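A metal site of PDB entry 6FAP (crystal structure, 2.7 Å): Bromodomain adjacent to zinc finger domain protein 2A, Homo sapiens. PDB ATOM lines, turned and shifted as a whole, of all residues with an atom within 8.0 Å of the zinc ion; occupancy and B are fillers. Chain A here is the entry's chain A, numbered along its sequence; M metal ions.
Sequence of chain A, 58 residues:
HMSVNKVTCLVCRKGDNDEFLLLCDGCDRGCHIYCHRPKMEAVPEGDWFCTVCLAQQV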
ATOM      1  N   THR A   8      22.023 -18.014  -4.292  1.00  0.00           N
ATOM      2  CA  THR A   8      22.243 -17.945  -2.848  1.00  0.00           C
ATOM      3  C   THR A   8      21.345 -18.906  -2.086  1.00  0.00           C
ATOM      4  O   THR A   8      20.332 -19.393  -2.603  1.00  0.00           O
ATOM      5  CB  THR A   8      22.011 -16.527  -2.306  1.00  0.00           C
ATOM      6  OG1 THR A   8      20.635 -16.154  -2.501  1.00  0.00           O
ATOM      7  CG2 THR A   8      22.922 -15.518  -3.002  1.00  0.00           C
ATOM      8  N   CYS A   9      21.698 -19.130  -0.827  1.00  0.00           N
ATOM      9  CA  CYS A   9      21.005 -20.073   0.031  1.00  0.00           C
ATOM     10  C   CYS A   9      19.892 -19.356   0.796  1.00  0.00           C
ATOM     11  O   CYS A   9      20.117 -18.287   1.367  1.00  0.00           O
ATOM     12  CB  CYS A   9      22.014 -20.708   0.994  1.00  0.00           C
ATOM     13  SG  CYS A   9      21.331 -21.603   2.407  1.00  0.00           S
ATOM     14  N   LEU A  10      18.689 -19.925   0.767  1.00  0.00           N
ATOM     15  CA  LEU A  10      17.510 -19.287   1.371  1.00  0.00           C
ATOM     16  C   LEU A  10      17.670 -19.097   2.876  1.00  0.00           C
ATOM     17  O   LEU A  10      17.196 -18.108   3.431  1.00  0.00           O
ATOM     18  CB  LEU A  10      16.254 -20.115   1.099  1.00  0.00           C
ATOM     19  CG  LEU A  10      15.755 -20.163  -0.347  1.00  0.00           C
ATOM     20  CD1 LEU A  10      14.768 -21.302  -0.543  1.00  0.00           C
ATOM     21  CD2 LEU A  10      15.138 -18.838  -0.753  1.00  0.00           C
ATOM     22  N   VAL A  11      18.321 -20.057   3.529  1.00  0.00           N
ATOM     23  CA  VAL A  11      18.437 -20.054   4.989  1.00  0.00           C
ATOM     24  C   VAL A  11      19.427 -18.994   5.473  1.00  0.00           C
ATOM     25  O   VAL A  11      19.073 -18.127   6.264  1.00  0.00           O
ATOM     26  CB  VAL A  11      18.883 -21.436   5.507  1.00  0.00           C
ATOM     27  CG1 VAL A  11      19.000 -21.431   7.037  1.00  0.00           C
ATOM     28  CG2 VAL A  11      17.910 -22.514   5.049  1.00  0.00           C
ATOM     29  N   CYS A  12      20.663 -19.064   4.969  1.00  0.00           N
ATOM     30  CA  CYS A  12      21.759 -18.249   5.505  1.00  0.00           C
ATOM     31  C   CYS A  12      22.131 -17.059   4.599  1.00  0.00           C
ATOM     32  O   CYS A  12      22.956 -16.226   4.989  1.00  0.00           O
ATOM     33  CB  CYS A  12      22.998 -19.130   5.732  1.00  0.00           C
ATOM     34  SG  CYS A  12      23.815 -19.681   4.224  1.00  0.00           S
ATOM     35  N   ARG A  13      21.577 -17.013   3.392  1.00  0.00           N
ATOM     36  CA  ARG A  13      21.725 -15.862   2.480  1.00  0.00           C
ATOM     37  C   ARG A  13      23.156 -15.650   1.971  1.00  0.00           C
ATOM     38  O   ARG A  13      23.494 -14.561   1.498  1.00  0.00           O
ATOM     39  CB  ARG A  13      21.198 -14.569   3.134  1.00  0.00           C
ATOM     40  CG  ARG A  13      19.704 -14.588   3.455  1.00  0.00           C
ATOM     41  CD  ARG A  13      18.856 -14.440   2.201  1.00  0.00           C
ATOM     42  N   LYS A  14      23.990 -16.687   2.039  1.00  0.00           N
ATOM     43  CA  LYS A  14      25.311 -16.671   1.399  1.00  0.00           C
ATOM     44  C   LYS A  14      25.322 -17.643   0.207  1.00  0.00           C
ATOM     45  O   LYS A  14      24.482 -18.547   0.120  1.00  0.00           O
ATOM     46  CB  LYS A  14      26.405 -17.063   2.397  1.00  0.00           C
ATOM     47  CG  LYS A  14      26.410 -16.235   3.677  1.00  0.00           C
ATOM     48  N   GLY A  15      26.260 -17.424  -0.707  1.00  0.00           N
ATOM     49  CA  GLY A  15      26.394 -18.261  -1.897  1.00  0.00           C
ATOM     50  C   GLY A  15      27.808 -18.770  -2.080  1.00  0.00           C
ATOM     51  O   GLY A  15      28.387 -18.673  -3.165  1.00  0.00           O
ATOM     52  N   ASP A  16      28.379 -19.327  -1.009  1.00  0.00           N
ATOM     53  CA  ASP A  16      29.697 -19.943  -1.040  1.00  0.00           C
ATOM     54  C   ASP A  16      29.568 -21.451  -0.805  1.00  0.00           C
ATOM     55  O   ASP A  16      28.465 -21.953  -0.611  1.00  0.00           O
ATOM     56  CB  ASP A  16      30.619 -19.310   0.001  1.00  0.00           C
ATOM     57  CG  ASP A  16      30.100 -19.484   1.421  1.00  0.00           C
ATOM     58  OD1 ASP A  16      28.877 -19.338   1.643  1.00  0.00           O
ATOM     59  OD2 ASP A  16      30.919 -19.762   2.323  1.00  0.00           O
ATOM     60  N   PHE A  20      28.164 -27.696  -2.136  1.00  0.00           N
ATOM     61  CA  PHE A  20      27.156 -28.174  -1.186  1.00  0.00           C
ATOM     62  C   PHE A  20      25.772 -27.538  -1.387  1.00  0.00           C
ATOM     63  O   PHE A  20      24.899 -27.652  -0.529  1.00  0.00           O
ATOM     64  CB  PHE A  20      27.617 -27.899   0.247  1.00  0.00           C
ATOM     65  CG  PHE A  20      28.826 -28.684   0.654  1.00  0.00           C
ATOM     66  CD1 PHE A  20      30.100 -28.214   0.381  1.00  0.00           C
ATOM     67  CD2 PHE A  20      28.687 -29.894   1.317  1.00  0.00           C
ATOM     68  CE1 PHE A  20      31.213 -28.933   0.759  1.00  0.00           C
ATOM     69  CE2 PHE A  20      29.800 -30.625   1.690  1.00  0.00           C
ATOM     70  CZ  PHE A  20      31.063 -30.135   1.424  1.00  0.00           C
ATOM     71  N   LEU A  21      25.574 -26.912  -2.551  1.00  0.00           N
ATOM     72  CA  LEU A  21      24.465 -25.978  -2.728  1.00  0.00           C
ATOM     73  C   LEU A  21      23.401 -26.579  -3.655  1.00  0.00           C
ATOM     74  O   LEU A  21      23.608 -26.659  -4.867  1.00  0.00           O
ATOM     75  CB  LEU A  21      24.992 -24.666  -3.306  1.00  0.00           C
ATOM     76  CG  LEU A  21      24.032 -23.477  -3.384  1.00  0.00           C
ATOM     77  CD1 LEU A  21      23.175 -23.365  -2.143  1.00  0.00           C
ATOM     78  CD2 LEU A  21      24.821 -22.197  -3.615  1.00  0.00           C
ATOM     79  N   GLY A  30      18.092 -21.807  -3.994  1.00  0.00           N
ATOM     80  CA  GLY A  30      19.005 -22.868  -3.556  1.00  0.00           C
ATOM     81  C   GLY A  30      19.086 -23.042  -2.053  1.00  0.00           C
ATOM     82  O   GLY A  30      18.550 -22.238  -1.286  1.00  0.00           O
ATOM     83  N   CYS A  31      19.750 -24.112  -1.637  1.00  0.00           N
ATOM     84  CA  CYS A  31      19.977 -24.371  -0.213  1.00  0.00           C
ATOM     85  C   CYS A  31      21.256 -25.180  -0.014  1.00  0.00           C
ATOM     86  O   CYS A  31      21.466 -26.183  -0.691  1.00  0.00           O
ATOM     87  CB  CYS A  31      18.791 -25.118   0.397  1.00  0.00           C
ATOM     88  SG  CYS A  31      18.631 -24.966   2.196  1.00  0.00           S
ATOM     89  N   HIS A  32      22.114 -24.737   0.898  1.00  0.00           N
ATOM     90  CA  HIS A  32      23.194 -25.578   1.409  1.00  0.00           C
ATOM     91  C   HIS A  32      22.579 -26.800   2.051  1.00  0.00           C
ATOM     92  O   HIS A  32      21.638 -26.684   2.837  1.00  0.00           O
ATOM     93  CB  HIS A  32      24.004 -24.844   2.472  1.00  0.00           C
ATOM     94  CG  HIS A  32      24.768 -23.673   1.948  1.00  0.00           C
ATOM     95  ND1 HIS A  32      24.533 -22.390   2.391  1.00  0.00           N
ATOM     96  CD2 HIS A  32      25.774 -23.592   1.050  1.00  0.00           C
ATOM     97  CE1 HIS A  32      25.378 -21.563   1.788  1.00  0.00           C
ATOM     98  NE2 HIS A  32      26.128 -22.264   0.964  1.00  0.00           N
ATOM     99  N   ILE A  33      23.137 -27.979   1.768  1.00  0.00           N
ATOM    100  CA  ILE A  33      22.650 -29.197   2.414  1.00  0.00           C
ATOM    101  C   ILE A  33      22.842 -29.149   3.927  1.00  0.00           C
ATOM    102  O   ILE A  33      22.031 -29.688   4.684  1.00  0.00           O
ATOM    103  CB  ILE A  33      23.281 -30.484   1.832  1.00  0.00           C
ATOM    104  CG1 ILE A  33      24.786 -30.524   2.047  1.00  0.00           C
ATOM    105  CG2 ILE A  33      22.949 -30.619   0.348  1.00  0.00           C
ATOM    106  CD1 ILE A  33      25.401 -31.870   1.703  1.00  0.00           C
ATOM    107  N   TYR A  34      23.891 -28.449   4.372  1.00  0.00           N
ATOM    108  CA  TYR A  34      24.174 -28.329   5.801  1.00  0.00           C
ATOM    109  C   TYR A  34      23.272 -27.313   6.533  1.00  0.00           C
ATOM    110  O   TYR A  34      23.203 -27.324   7.756  1.00  0.00           O
ATOM    111  CB  TYR A  34      25.655 -28.018   6.055  1.00  0.00           C
ATOM    112  CG  TYR A  34      26.218 -26.832   5.299  1.00  0.00           C
ATOM    113  CD1 TYR A  34      26.020 -25.532   5.753  1.00  0.00           C
ATOM    114  CD2 TYR A  34      27.041 -27.012   4.189  1.00  0.00           C
ATOM    115  CE1 TYR A  34      26.562 -24.441   5.099  1.00  0.00           C
ATOM    116  CE2 TYR A  34      27.591 -25.932   3.525  1.00  0.00           C
ATOM    117  CZ  TYR A  34      27.351 -24.647   3.980  1.00  0.00           C
ATOM    118  OH  TYR A  34      27.905 -23.563   3.325  1.00  0.00           O
ATOM    119  N   CYS A  35      22.577 -26.461   5.773  1.00  0.00           N
ATOM    120  CA  CYS A  35      21.577 -25.552   6.361  1.00  0.00           C
ATOM    121  C   CYS A  35      20.186 -26.202   6.426  1.00  0.00           C
ATOM    122  O   CYS A  35      19.341 -25.773   7.208  1.00  0.00           O
ATOM    123  CB  CYS A  35      21.517 -24.247   5.566  1.00  0.00           C
ATOM    124  SG  CYS A  35      22.968 -23.159   5.737  1.00  0.00           S
ATOM    125  N   HIS A  36      19.956 -27.232   5.612  1.00  0.00           N
ATOM    126  CA  HIS A  36      18.645 -27.854   5.511  1.00  0.00           C
ATOM    127  C   HIS A  36      18.266 -28.594   6.793  1.00  0.00           C
ATOM    128  O   HIS A  36      19.088 -29.321   7.355  1.00  0.00           O
ATOM    129  CB  HIS A  36      18.614 -28.827   4.325  1.00  0.00           C
ATOM    130  CG  HIS A  36      17.232 -29.194   3.867  1.00  0.00           C
ATOM    131  ND1 HIS A  36      16.498 -30.203   4.441  1.00  0.00           N
ATOM    132  CD2 HIS A  36      16.472 -28.700   2.846  1.00  0.00           C
ATOM    133  CE1 HIS A  36      15.335 -30.313   3.813  1.00  0.00           C
ATOM    134  NE2 HIS A  36      15.297 -29.418   2.842  1.00  0.00           N
HETATM  135 ZN    ZN M   1      23.185 -21.887   3.797  1.00  0.00          ZN
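The zinc ion is bound by a ring nitrogen (ND1) of His 32 (2.0 Å), the side-chain sulfur of Cys 35 (2.3 Å), the side-chain sulfur of Cys 12 (2.3 Å) and the side-chain sulfur of Cys 9 (2.3 Å).
Of the 18 residues printed, 4 come within 4 Å of the zinc ion.
The nearest printed residue that does not touch the zinc ion is Tyr 34 (4.4 Å).
The side-chain hydroxyl of Tyr 34 lies close to a ring nitrogen (NE2) of His 32 (3.2 Å).
A ring nitrogen (NE2) of His 32 sits at hydrogen-bond distance from the backbone carbonyl oxygen (O) of Asp 16, at 2.8 Å.
The backbone NH of Lys 14 lies close to the side-chain sulfur of Cys 12, at 3.7 Å.
SG of Cys 9 sits close to N of Val 11, at 3.6 Å.
N of Cys 9 sits at hydrogen-bond distance from O of Lys 14.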
